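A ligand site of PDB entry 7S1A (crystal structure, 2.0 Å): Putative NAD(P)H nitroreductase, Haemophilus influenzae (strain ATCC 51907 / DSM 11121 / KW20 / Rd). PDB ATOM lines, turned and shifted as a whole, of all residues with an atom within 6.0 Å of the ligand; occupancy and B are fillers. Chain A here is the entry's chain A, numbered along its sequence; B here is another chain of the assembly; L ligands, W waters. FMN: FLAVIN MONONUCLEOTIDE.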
ATOM      1  N   ARG A  19      -6.825  -8.321  -3.078  1.00  0.00           N
ATOM      2  CA  ARG A  19      -7.107  -8.362  -4.514  1.00  0.00           C
ATOM      3  C   ARG A  19      -7.737  -9.704  -4.837  1.00  0.00           C
ATOM      4  O   ARG A  19      -7.073 -10.742  -4.732  1.00  0.00           O
ATOM      5  CB  ARG A  19      -5.821  -8.150  -5.317  1.00  0.00           C
ATOM      6  CG  ARG A  19      -6.012  -7.725  -6.784  1.00  0.00           C
ATOM      7  CD  ARG A  19      -6.136  -8.913  -7.745  1.00  0.00           C
ATOM      8  NE  ARG A  19      -5.532 -10.136  -7.226  1.00  0.00           N
ATOM      9  CZ  ARG A  19      -5.979 -11.354  -7.498  1.00  0.00           C
ATOM     10  NH1 ARG A  19      -6.988 -11.545  -8.346  1.00  0.00           N
ATOM     11  NH2 ARG A  19      -5.433 -12.405  -6.895  1.00  0.00           N
ATOM     12  N   SER A  20      -8.997  -9.699  -5.235  1.00  0.00           N
ATOM     13  CA  SER A  20      -9.658 -10.919  -5.706  1.00  0.00           C
ATOM     14  C   SER A  20     -10.223 -10.723  -7.108  1.00  0.00           C
ATOM     15  O   SER A  20     -10.461  -9.597  -7.554  1.00  0.00           O
ATOM     16  CB  SER A  20     -10.755 -11.345  -4.739  1.00  0.00           C
ATOM     17  OG  SER A  20     -10.156 -11.796  -3.528  1.00  0.00           O
ATOM     18  N   SER A  21     -10.467 -11.853  -7.780  1.00  0.00           N
ATOM     19  CA  SER A  21     -11.112 -11.877  -9.089  1.00  0.00           C
ATOM     20  C   SER A  21     -12.629 -11.809  -8.906  1.00  0.00           C
ATOM     21  O   SER A  21     -13.254 -12.760  -8.419  1.00  0.00           O
ATOM     22  CB  SER A  21     -10.719 -13.134  -9.855  1.00  0.00           C
ATOM     23  OG  SER A  21      -9.356 -13.080 -10.262  1.00  0.00           O
ATOM     24  N   THR A  22     -13.234 -10.695  -9.314  1.00  0.00           N
ATOM     25  CA  THR A  22     -14.662 -10.470  -9.135  1.00  0.00           C
ATOM     26  C   THR A  22     -15.424 -10.897 -10.392  1.00  0.00           C
ATOM     27  O   THR A  22     -15.128 -10.423 -11.502  1.00  0.00           O
ATOM     28  CB  THR A  22     -14.914  -9.007  -8.790  1.00  0.00           C
ATOM     29  OG1 THR A  22     -14.396  -8.186  -9.835  1.00  0.00           O
ATOM     30  CG2 THR A  22     -14.175  -8.654  -7.541  1.00  0.00           C
ATOM     31  N   ARG A  23     -16.391 -11.805 -10.219  1.00  0.00           N
ATOM     32  CA  ARG A  23     -17.212 -12.292 -11.316  1.00  0.00           C
ATOM     33  C   ARG A  23     -18.527 -11.545 -11.437  1.00  0.00           C
ATOM     34  O   ARG A  23     -19.178 -11.638 -12.477  1.00  0.00           O
ATOM     35  CB  ARG A  23     -17.532 -13.786 -11.145  1.00  0.00           C
ATOM     36  CG  ARG A  23     -16.414 -14.728 -11.590  1.00  0.00           C
ATOM     37  CD  ARG A  23     -15.258 -14.656 -10.630  1.00  0.00           C
ATOM     38  NE  ARG A  23     -14.082 -15.272 -11.223  1.00  0.00           N
ATOM     39  CZ  ARG A  23     -13.368 -16.238 -10.663  1.00  0.00           C
ATOM     40  NH1 ARG A  23     -13.661 -16.704  -9.454  1.00  0.00           N
ATOM     41  NH2 ARG A  23     -12.348 -16.749 -11.335  1.00  0.00           N
ATOM     42  N   TRP A  74     -17.189 -16.419 -22.828  1.00  0.00           N
ATOM     43  CA  TRP A  74     -17.861 -17.072 -21.705  1.00  0.00           C
ATOM     44  C   TRP A  74     -17.181 -16.770 -20.367  1.00  0.00           C
ATOM     45  O   TRP A  74     -17.829 -16.796 -19.320  1.00  0.00           O
ATOM     46  CB  TRP A  74     -17.897 -18.584 -21.938  1.00  0.00           C
ATOM     47  CG  TRP A  74     -16.541 -19.209 -22.177  1.00  0.00           C
ATOM     48  CD1 TRP A  74     -15.938 -19.442 -23.382  1.00  0.00           C
ATOM     49  CD2 TRP A  74     -15.626 -19.676 -21.167  1.00  0.00           C
ATOM     50  NE1 TRP A  74     -14.711 -20.038 -23.179  1.00  0.00           N
ATOM     51  CE2 TRP A  74     -14.497 -20.183 -21.839  1.00  0.00           C
ATOM     52  CE3 TRP A  74     -15.661 -19.720 -19.765  1.00  0.00           C
ATOM     53  CZ2 TRP A  74     -13.404 -20.729 -21.145  1.00  0.00           C
ATOM     54  CZ3 TRP A  74     -14.585 -20.254 -19.092  1.00  0.00           C
ATOM     55  CH2 TRP A  74     -13.468 -20.757 -19.772  1.00  0.00           C
ATOM     56  N   GLY A  75     -15.875 -16.480 -20.385  1.00  0.00           N
ATOM     57  CA  GLY A  75     -15.193 -16.179 -19.150  1.00  0.00           C
ATOM     58  C   GLY A  75     -15.618 -14.868 -18.507  1.00  0.00           C
ATOM     59  O   GLY A  75     -15.291 -14.646 -17.340  1.00  0.00           O
ATOM     60  N   MET A  76     -16.304 -14.008 -19.232  1.00  0.00           N
ATOM     61  CA  MET A  76     -16.672 -12.712 -18.674  1.00  0.00           C
ATOM     62  C   MET A  76     -18.067 -12.282 -19.099  1.00  0.00           C
ATOM     63  O   MET A  76     -18.385 -11.090 -19.036  1.00  0.00           O
ATOM     64  CB  MET A  76     -15.645 -11.656 -19.087  1.00  0.00           C
ATOM     65  CG  MET A  76     -15.359 -11.578 -20.580  1.00  0.00           C
ATOM     66  SD  MET A  76     -14.282 -10.012 -21.025  1.00  0.00           S
ATOM     67  CE  MET A  76     -14.009 -10.351 -22.914  1.00  0.00           C
ATOM     68  N   GLN A  79     -19.892 -10.324 -16.791  1.00  0.00           N
ATOM     69  CA  GLN A  79     -19.092  -9.138 -16.466  1.00  0.00           C
ATOM     70  C   GLN A  79     -19.123  -8.095 -17.581  1.00  0.00           C
ATOM     71  O   GLN A  79     -18.999  -6.893 -17.311  1.00  0.00           O
ATOM     72  CB  GLN A  79     -17.649  -9.555 -16.201  1.00  0.00           C
ATOM     73  CG  GLN A  79     -17.455 -10.731 -15.227  1.00  0.00           C
ATOM     74  CD  GLN A  79     -15.970 -11.084 -15.072  1.00  0.00           C
ATOM     75  OE1 GLN A  79     -15.603 -12.258 -14.888  1.00  0.00           O
ATOM     76  NE2 GLN A  79     -15.107 -10.076 -15.150  1.00  0.00           N
ATOM     77  N   TYR A 149       1.752  -9.962 -19.518  1.00  0.00           N
ATOM     78  CA  TYR A 149       1.169 -10.439 -18.268  1.00  0.00           C
ATOM     79  C   TYR A 149       1.745  -9.692 -17.081  1.00  0.00           C
ATOM     80  O   TYR A 149       1.124  -9.687 -16.022  1.00  0.00           O
ATOM     81  CB  TYR A 149       1.357 -11.942 -18.116  1.00  0.00           C
ATOM     82  CG  TYR A 149       0.251 -12.761 -18.823  1.00  0.00           C
ATOM     83  CD1 TYR A 149       0.058 -12.652 -20.192  1.00  0.00           C
ATOM     84  CD2 TYR A 149      -0.557 -13.662 -18.110  1.00  0.00           C
ATOM     85  CE1 TYR A 149      -0.946 -13.397 -20.866  1.00  0.00           C
ATOM     86  CE2 TYR A 149      -1.571 -14.405 -18.769  1.00  0.00           C
ATOM     87  CZ  TYR A 149      -1.739 -14.264 -20.149  1.00  0.00           C
ATOM     88  OH  TYR A 149      -2.721 -14.981 -20.820  1.00  0.00           O
ATOM     89  N   LEU A 152      -0.435  -6.761 -16.953  1.00  0.00           N
ATOM     90  CA  LEU A 152      -1.682  -7.293 -16.411  1.00  0.00           C
ATOM     91  C   LEU A 152      -1.637  -7.315 -14.889  1.00  0.00           C
ATOM     92  O   LEU A 152      -2.500  -6.753 -14.219  1.00  0.00           O
ATOM     93  CB  LEU A 152      -1.934  -8.702 -16.939  1.00  0.00           C
ATOM     94  CG  LEU A 152      -3.113  -9.361 -16.216  1.00  0.00           C
ATOM     95  CD1 LEU A 152      -4.338  -8.614 -16.613  1.00  0.00           C
ATOM     96  CD2 LEU A 152      -3.237 -10.859 -16.545  1.00  0.00           C
ATOM     97  N   LEU A 156      -3.788  -5.027 -12.015  1.00  0.00           N
ATOM     98  CA  LEU A 156      -4.632  -5.567 -10.957  1.00  0.00           C
ATOM     99  C   LEU A 156      -4.189  -5.033  -9.601  1.00  0.00           C
ATOM    100  O   LEU A 156      -5.012  -4.582  -8.779  1.00  0.00           O
ATOM    101  CB  LEU A 156      -4.589  -7.087 -10.968  1.00  0.00           C
ATOM    102  CG  LEU A 156      -4.815  -7.818 -12.291  1.00  0.00           C
ATOM    103  CD1 LEU A 156      -4.667  -9.289 -12.009  1.00  0.00           C
ATOM    104  CD2 LEU A 156      -6.218  -7.510 -12.839  1.00  0.00           C
ATOM    105  N   CYS A 167     -10.816  -8.302 -12.565  1.00  0.00           N
ATOM    106  CA  CYS A 167     -10.802  -9.723 -12.923  1.00  0.00           C
ATOM    107  C   CYS A 167      -9.999  -9.972 -14.202  1.00  0.00           C
ATOM    108  O   CYS A 167     -10.379  -9.491 -15.272  1.00  0.00           O
ATOM    109  CB  CYS A 167     -12.221 -10.271 -13.116  1.00  0.00           C
ATOM    110  SG  CYS A 167     -12.280 -12.081 -13.205  1.00  0.00           S
ATOM    111  N   PRO A 168      -8.906 -10.719 -14.117  1.00  0.00           N
ATOM    112  CA  PRO A 168      -8.173 -11.093 -15.343  1.00  0.00           C
ATOM    113  C   PRO A 168      -8.928 -12.154 -16.122  1.00  0.00           C
ATOM    114  O   PRO A 168      -9.567 -13.038 -15.553  1.00  0.00           O
ATOM    115  CB  PRO A 168      -6.849 -11.638 -14.811  1.00  0.00           C
ATOM    116  CG  PRO A 168      -7.168 -12.109 -13.429  1.00  0.00           C
ATOM    117  CD  PRO A 168      -8.261 -11.241 -12.898  1.00  0.00           C
ATOM    118  N   ILE A 169      -8.852 -12.070 -17.441  1.00  0.00           N
ATOM    119  CA  ILE A 169      -9.751 -12.823 -18.303  1.00  0.00           C
ATOM    120  C   ILE A 169      -8.951 -13.475 -19.427  1.00  0.00           C
ATOM    121  O   ILE A 169      -8.359 -12.779 -20.261  1.00  0.00           O
ATOM    122  CB  ILE A 169     -10.872 -11.930 -18.854  1.00  0.00           C
ATOM    123  CG1 ILE A 169     -11.768 -11.446 -17.708  1.00  0.00           C
ATOM    124  CG2 ILE A 169     -11.739 -12.679 -19.821  1.00  0.00           C
ATOM    125  CD1 ILE A 169     -12.382 -12.576 -16.929  1.00  0.00           C
ATOM    126  N   GLU A 170      -8.940 -14.810 -19.450  1.00  0.00           N
ATOM    127  CA  GLU A 170      -8.549 -15.595 -20.612  1.00  0.00           C
ATOM    128  C   GLU A 170      -9.726 -16.336 -21.240  1.00  0.00           C
ATOM    129  O   GLU A 170      -9.561 -16.950 -22.296  1.00  0.00           O
ATOM    130  CB  GLU A 170      -7.479 -16.626 -20.238  1.00  0.00           C
ATOM    131  CG  GLU A 170      -6.072 -16.110 -20.314  1.00  0.00           C
ATOM    132  CD  GLU A 170      -5.059 -17.092 -19.742  1.00  0.00           C
ATOM    133  OE1 GLU A 170      -5.420 -18.249 -19.477  1.00  0.00           O
ATOM    134  OE2 GLU A 170      -3.885 -16.698 -19.585  1.00  0.00           O
ATOM    135  N   GLY A 171     -10.908 -16.255 -20.625  1.00  0.00           N
ATOM    136  CA  GLY A 171     -12.041 -17.082 -20.998  1.00  0.00           C
ATOM    137  C   GLY A 171     -12.797 -16.586 -22.209  1.00  0.00           C
ATOM    138  O   GLY A 171     -13.973 -16.246 -22.128  1.00  0.00           O
ATOM    139  N   PHE A 172     -12.131 -16.574 -23.360  1.00  0.00           N
ATOM    140  CA  PHE A 172     -12.813 -16.207 -24.597  1.00  0.00           C
ATOM    141  C   PHE A 172     -12.101 -16.917 -25.733  1.00  0.00           C
ATOM    142  O   PHE A 172     -10.975 -17.377 -25.587  1.00  0.00           O
ATOM    143  CB  PHE A 172     -12.838 -14.688 -24.798  1.00  0.00           C
ATOM    144  CG  PHE A 172     -11.467 -14.057 -24.743  1.00  0.00           C
ATOM    145  CD1 PHE A 172     -10.936 -13.635 -23.540  1.00  0.00           C
ATOM    146  CD2 PHE A 172     -10.725 -13.900 -25.912  1.00  0.00           C
ATOM    147  CE1 PHE A 172      -9.668 -13.052 -23.482  1.00  0.00           C
ATOM    148  CE2 PHE A 172      -9.468 -13.314 -25.862  1.00  0.00           C
ATOM    149  CZ  PHE A 172      -8.940 -12.900 -24.632  1.00  0.00           C
ATOM    150  N   VAL A 196      -4.348 -10.925 -23.489  1.00  0.00           N
ATOM    151  CA  VAL A 196      -5.155 -11.212 -22.291  1.00  0.00           C
ATOM    152  C   VAL A 196      -6.054 -10.012 -22.020  1.00  0.00           C
ATOM    153  O   VAL A 196      -5.848  -8.933 -22.570  1.00  0.00           O
ATOM    154  CB  VAL A 196      -4.256 -11.531 -21.080  1.00  0.00           C
ATOM    155  CG1 VAL A 196      -3.403 -10.321 -20.682  1.00  0.00           C
ATOM    156  CG2 VAL A 196      -5.089 -12.039 -19.901  1.00  0.00           C
ATOM    157  N   ALA A 208     -14.321 -13.467  -1.895  1.00  0.00           N
ATOM    158  CA  ALA A 208     -14.196 -14.889  -1.588  1.00  0.00           C
ATOM    159  C   ALA A 208     -12.841 -15.184  -0.968  1.00  0.00           C
ATOM    160  O   ALA A 208     -11.884 -14.422  -1.094  1.00  0.00           O
ATOM    161  CB  ALA A 208     -14.384 -15.723  -2.852  1.00  0.00           C
ATOM    162  N   LYS A 210      -9.255 -17.185  -0.357  1.00  0.00           N
ATOM    163  CA  LYS A 210      -8.203 -17.550  -1.281  1.00  0.00           C
ATOM    164  C   LYS A 210      -7.860 -19.022  -1.122  1.00  0.00           C
ATOM    165  O   LYS A 210      -7.573 -19.479  -0.012  1.00  0.00           O
ATOM    166  CB  LYS A 210      -6.945 -16.710  -1.065  1.00  0.00           C
ATOM    167  CG  LYS A 210      -7.190 -15.200  -1.061  1.00  0.00           C
ATOM    168  CD  LYS A 210      -5.928 -14.405  -1.389  1.00  0.00           C
ATOM    169  CE  LYS A 210      -5.891 -13.969  -2.861  1.00  0.00           C
ATOM    170  NZ  LYS A 210      -7.016 -13.066  -3.255  1.00  0.00           N
ATOM    171  N   SER A 211      -7.900 -19.756  -2.221  1.00  0.00           N
ATOM    172  CA  SER A 211      -7.414 -21.127  -2.238  1.00  0.00           C
ATOM    173  C   SER A 211      -6.092 -21.132  -2.984  1.00  0.00           C
ATOM    174  O   SER A 211      -6.061 -21.065  -4.210  1.00  0.00           O
ATOM    175  CB  SER A 211      -8.437 -22.057  -2.891  1.00  0.00           C
ATOM    176  OG  SER A 211      -8.041 -23.400  -2.734  1.00  0.00           O
ATOM    177  N   ARG A 212      -4.982 -21.171  -2.238  1.00  0.00           N
ATOM    178  CA  ARG A 212      -3.655 -21.299  -2.825  1.00  0.00           C
ATOM    179  C   ARG A 212      -2.943 -22.522  -2.269  1.00  0.00           C
ATOM    180  O   ARG A 212      -3.241 -22.983  -1.163  1.00  0.00           O
ATOM    181  CB  ARG A 212      -2.777 -20.058  -2.564  1.00  0.00           C
ATOM    182  CG  ARG A 212      -3.202 -18.786  -3.253  1.00  0.00           C
ATOM    183  CD  ARG A 212      -3.154 -18.872  -4.771  1.00  0.00           C
ATOM    184  NE  ARG A 212      -3.382 -17.546  -5.331  1.00  0.00           N
ATOM    185  CZ  ARG A 212      -4.581 -17.012  -5.533  1.00  0.00           C
ATOM    186  NH1 ARG A 212      -5.697 -17.694  -5.317  1.00  0.00           N
ATOM    187  NH2 ARG A 212      -4.669 -15.752  -5.953  1.00  0.00           N
ATOM    188  N   LEU B  45       0.390 -15.739  -3.625  1.00  0.00           N
ATOM    189  CA  LEU B  45      -0.932 -15.125  -3.613  1.00  0.00           C
ATOM    190  C   LEU B  45      -1.372 -14.620  -4.988  1.00  0.00           C
ATOM    191  O   LEU B  45      -2.521 -14.188  -5.136  1.00  0.00           O
ATOM    192  CB  LEU B  45      -0.968 -13.966  -2.599  1.00  0.00           C
ATOM    193  CG  LEU B  45      -0.748 -14.264  -1.101  1.00  0.00           C
ATOM    194  CD1 LEU B  45      -1.154 -13.083  -0.232  1.00  0.00           C
ATOM    195  CD2 LEU B  45      -1.498 -15.503  -0.694  1.00  0.00           C
ATOM    196  N   SER B  46      -0.503 -14.691  -5.995  1.00  0.00           N
ATOM    197  CA  SER B  46      -0.819 -14.152  -7.307  1.00  0.00           C
ATOM    198  C   SER B  46      -1.969 -14.921  -7.947  1.00  0.00           C
ATOM    199  O   SER B  46      -2.199 -16.097  -7.648  1.00  0.00           O
ATOM    200  CB  SER B  46       0.399 -14.185  -8.229  1.00  0.00           C
ATOM    201  OG  SER B  46       1.302 -13.148  -7.866  1.00  0.00           O
ATOM    202  N   PRO B  47      -2.739 -14.276  -8.809  1.00  0.00           N
ATOM    203  CA  PRO B  47      -3.831 -14.968  -9.501  1.00  0.00           C
ATOM    204  C   PRO B  47      -3.278 -15.758 -10.680  1.00  0.00           C
ATOM    205  O   PRO B  47      -2.190 -15.510 -11.166  1.00  0.00           O
ATOM    206  CB  PRO B  47      -4.718 -13.812  -9.973  1.00  0.00           C
ATOM    207  CG  PRO B  47      -3.735 -12.728 -10.265  1.00  0.00           C
ATOM    208  CD  PRO B  47      -2.688 -12.851  -9.188  1.00  0.00           C
ATOM    209  N   SER B  48      -4.075 -16.718 -11.149  1.00  0.00           N
ATOM    210  CA  SER B  48      -3.629 -17.535 -12.275  1.00  0.00           C
ATOM    211  C   SER B  48      -4.834 -18.108 -13.002  1.00  0.00           C
ATOM    212  O   SER B  48      -5.840 -18.416 -12.367  1.00  0.00           O
ATOM    213  CB  SER B  48      -2.709 -18.665 -11.815  1.00  0.00           C
ATOM    214  OG  SER B  48      -3.452 -19.558 -11.018  1.00  0.00           O
ATOM    215  N   SER B  49      -4.714 -18.255 -14.319  1.00  0.00           N
ATOM    216  CA  SER B  49      -5.773 -18.847 -15.121  1.00  0.00           C
ATOM    217  C   SER B  49      -6.252 -20.132 -14.463  1.00  0.00           C
ATOM    218  O   SER B  49      -5.435 -20.952 -14.057  1.00  0.00           O
ATOM    219  CB  SER B  49      -5.272 -19.134 -16.538  1.00  0.00           C
ATOM    220  OG  SER B  49      -6.324 -19.470 -17.416  1.00  0.00           O
ATOM    221  N   VAL B  50      -7.580 -20.255 -14.329  1.00  0.00           N
ATOM    222  CA  VAL B  50      -8.294 -21.405 -13.753  1.00  0.00           C
ATOM    223  C   VAL B  50      -7.647 -21.915 -12.472  1.00  0.00           C
ATOM    224  O   VAL B  50      -7.701 -23.112 -12.178  1.00  0.00           O
ATOM    225  CB  VAL B  50      -8.483 -22.555 -14.772  1.00  0.00           C
ATOM    226  CG1 VAL B  50      -9.399 -22.134 -15.935  1.00  0.00           C
ATOM    227  CG2 VAL B  50      -7.154 -23.114 -15.321  1.00  0.00           C
ATOM    228  N   GLY B  51      -7.103 -21.004 -11.665  1.00  0.00           N
ATOM    229  CA  GLY B  51      -6.528 -21.397 -10.375  1.00  0.00           C
ATOM    230  C   GLY B  51      -5.401 -22.395 -10.517  1.00  0.00           C
ATOM    231  O   GLY B  51      -5.207 -23.242  -9.645  1.00  0.00           O
ATOM    232  N   LYS B 109     -10.098 -26.543  -5.307  1.00  0.00           N
ATOM    233  CA  LYS B 109     -11.360 -25.822  -5.451  1.00  0.00           C
ATOM    234  C   LYS B 109     -12.535 -26.546  -4.819  1.00  0.00           C
ATOM    235  O   LYS B 109     -13.645 -26.005  -4.807  1.00  0.00           O
ATOM    236  CB  LYS B 109     -11.633 -25.544  -6.933  1.00  0.00           C
ATOM    237  CG  LYS B 109     -10.602 -24.643  -7.609  1.00  0.00           C
ATOM    238  CD  LYS B 109     -11.153 -24.045  -8.906  1.00  0.00           C
ATOM    239  CE  LYS B 109     -10.152 -23.098  -9.611  1.00  0.00           C
ATOM    240  NZ  LYS B 109      -9.771 -21.933  -8.755  1.00  0.00           N
ATOM    241  N   GLN B 147       1.522 -17.329 -16.775  1.00  0.00           N
ATOM    242  CA  GLN B 147       1.003 -17.122 -15.411  1.00  0.00           C
ATOM    243  C   GLN B 147       2.140 -16.804 -14.423  1.00  0.00           C
ATOM    244  O   GLN B 147       1.956 -15.991 -13.516  1.00  0.00           O
ATOM    245  CB  GLN B 147       0.218 -18.347 -14.939  1.00  0.00           C
ATOM    246  CG  GLN B 147      -0.689 -19.010 -15.992  1.00  0.00           C
ATOM    247  CD  GLN B 147      -1.778 -18.096 -16.518  1.00  0.00           C
ATOM    248  OE1 GLN B 147      -2.322 -17.260 -15.784  1.00  0.00           O
ATOM    249  NE2 GLN B 147      -2.107 -18.242 -17.805  1.00  0.00           N
ATOM    250  N   ILE B 150       3.048 -13.317 -13.884  1.00  0.00           N
ATOM    251  CA  ILE B 150       2.221 -12.582 -12.941  1.00  0.00           C
ATOM    252  C   ILE B 150       2.856 -12.627 -11.556  1.00  0.00           C
ATOM    253  O   ILE B 150       3.009 -11.592 -10.891  1.00  0.00           O
ATOM    254  CB  ILE B 150       0.785 -13.141 -12.940  1.00  0.00           C
ATOM    255  CG1 ILE B 150       0.206 -13.090 -14.338  1.00  0.00           C
ATOM    256  CG2 ILE B 150      -0.128 -12.391 -11.944  1.00  0.00           C
ATOM    257  CD1 ILE B 150      -1.279 -13.404 -14.365  1.00  0.00           C
HETATM  258  N1  FMN L   1     -11.709 -15.608 -14.036  1.00  0.00           N
HETATM  259  C2  FMN L   1     -12.862 -15.498 -14.746  1.00  0.00           C
HETATM  260  O2  FMN L   1     -13.931 -15.240 -14.186  1.00  0.00           O
HETATM  261  N3  FMN L   1     -12.902 -15.793 -16.081  1.00  0.00           N
HETATM  262  C4  FMN L   1     -11.768 -16.064 -16.798  1.00  0.00           C
HETATM  263  O4  FMN L   1     -11.843 -16.273 -18.003  1.00  0.00           O
HETATM  264  C4A FMN L   1     -10.528 -16.016 -16.115  1.00  0.00           C
HETATM  265  N5  FMN L   1      -9.399 -16.075 -16.797  1.00  0.00           N
HETATM  266  C5A FMN L   1      -8.253 -15.777 -16.102  1.00  0.00           C
HETATM  267  C6  FMN L   1      -7.062 -15.565 -16.821  1.00  0.00           C
HETATM  268  C7  FMN L   1      -5.908 -15.156 -16.183  1.00  0.00           C
HETATM  269  C7M FMN L   1      -4.646 -14.913 -16.965  1.00  0.00           C
HETATM  270  C8  FMN L   1      -5.895 -15.031 -14.773  1.00  0.00           C
HETATM  271  C8M FMN L   1      -4.619 -14.671 -14.051  1.00  0.00           C
HETATM  272  C9  FMN L   1      -7.027 -15.360 -14.056  1.00  0.00           C
HETATM  273  C9A FMN L   1      -8.224 -15.711 -14.699  1.00  0.00           C
HETATM  274  N10 FMN L   1      -9.408 -15.959 -14.004  1.00  0.00           N
HETATM  275  C10 FMN L   1     -10.602 -15.872 -14.689  1.00  0.00           C
HETATM  276  C1' FMN L   1      -9.435 -15.794 -12.536  1.00  0.00           C
HETATM  277  C2' FMN L   1      -8.846 -16.983 -11.795  1.00  0.00           C
HETATM  278  O2' FMN L   1      -9.661 -18.160 -11.935  1.00  0.00           O
HETATM  279  C3' FMN L   1      -8.566 -16.582 -10.335  1.00  0.00           C
HETATM  280  O3' FMN L   1      -7.601 -15.538 -10.330  1.00  0.00           O
HETATM  281  C4' FMN L   1      -8.078 -17.680  -9.382  1.00  0.00           C
HETATM  282  O4' FMN L   1      -9.072 -18.699  -9.213  1.00  0.00           O
HETATM  283  C5' FMN L   1      -7.619 -17.125  -8.041  1.00  0.00           C
HETATM  284  O5' FMN L   1      -8.615 -16.316  -7.343  1.00  0.00           O
HETATM  285  P   FMN L   1      -8.288 -14.792  -7.002  1.00  0.00           P
HETATM  286  O1P FMN L   1      -9.600 -14.187  -6.533  1.00  0.00           O
HETATM  287  O2P FMN L   1      -7.225 -14.817  -5.911  1.00  0.00           O
HETATM  288  O3P FMN L   1      -7.776 -14.190  -8.293  1.00  0.00           O
HETATM  289  O   HOH W   1     -10.450 -19.363 -14.361  1.00  0.00           O
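O of Pro 168 lies close to N5 of the ligand (3.3 Å). Ser 20 touches the ligand. CE2 of Tyr 149 touches C7M of the ligand (3.6 Å). CD1 of Ile 169 touches N3 of the ligand, 3.4 Å away. Pro 47 of chain B touches the ligand (CB to O3', 3.4 Å). Ser 48 of chain B touches the ligand (O to C2', 3.4 Å). N of Ser 49 of chain B touches C8 of the ligand, 3.5 Å away. Val 50 of chain B touches the ligand (N to O2', 3.8 Å). N of Gly 51 of chain B touches O2' of the ligand, at 3.8 Å. Gln 147 of chain B touches the ligand (OE1 to C7M, 3.5 Å). Ile 150 of chain B touches the ligand. Hydrophobic or aromatic side chains that line the ligand: Tyr 149, Pro 168, Ile 169, Pro 47 of chain B and Ile 150 of chain B. Of the 33 residues printed, 22 come within 4 Å of the ligand.
Water W1 lies within hydrogen-bond range of O2' of the ligand (2.8 Å) and N of Val 50 of chain B (3.0 Å).
The guanidinium group (NH2) of Arg 212 lies within hydrogen-bond range of the backbone carbonyl oxygen (O) of Leu 45 of chain B, at 2.8 Å. NE of Arg 212 lies within hydrogen-bond range of O of Ser 46 of chain B (3.0 Å). The backbone carbonyl oxygen (O) of Gly 171 sits at hydrogen-bond distance from the backbone NH (N) of Gly 75 (2.6 Å). OG of Ser 49 of chain B sits at hydrogen-bond distance from OE1 of Glu 170, at 2.6 Å. The side-chain carboxylate (OE2) of Glu 170 is in hydrogen-bond range of the side-chain amide nitrogen (NE2) of Gln 147 of chain B (3.0 Å). The side-chain amino group (NZ) of Lys 210 sits at hydrogen-bond distance from the side-chain hydroxyl (OG) of Ser 20. The backbone NH (N) of Ser 49 of chain B lies within hydrogen-bond range of the side-chain amide oxygen (OE1) of Gln 147 of chain B, 3.0 Å away. OE1 of Gln 79 is in hydrogen-bond range of SG of Cys 167, at 3.7 Å.
An oxygen (O2P) of the ligand lies within salt-bridge range of the guanidinium group (NH2) of Arg 212 (2.7 Å). The backbone NH (N) of Ser 21 sits at hydrogen-bond distance from an oxygen (O1P) of the ligand (2.8 Å). OG of Ser 21 sits at hydrogen-bond distance from O3P of the ligand (2.8 Å). O3P of the ligand is in salt-bridge range of NH1 of Arg 19 (2.8 Å). N of Gly 171 lies within hydrogen-bond range of O4 of the ligand. A nitrogen (N3) of the ligand sits at hydrogen-bond distance from the backbone carbonyl oxygen of Gly 75, at 2.9 Å. An oxygen (O2) of the ligand is in hydrogen-bond range of the guanidinium group of Arg 23 (3.0 Å). N5 of the ligand lies within hydrogen-bond range of N of Glu 170 (3.0 Å). An oxygen (O2P) of the ligand lies within salt-bridge range of the side-chain amino group (NZ) of Lys 210 (3.2 Å). NZ of Lys 109 of chain B is in hydrogen-bond range of O4' of the ligand (3.3 Å). The side-chain amide oxygen of Gln 79 sits close to an oxygen (O2) of the ligand (3.5 Å). SG of Cys 167 sits at hydrogen-bond distance from N1 of the ligand (3.7 Å).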
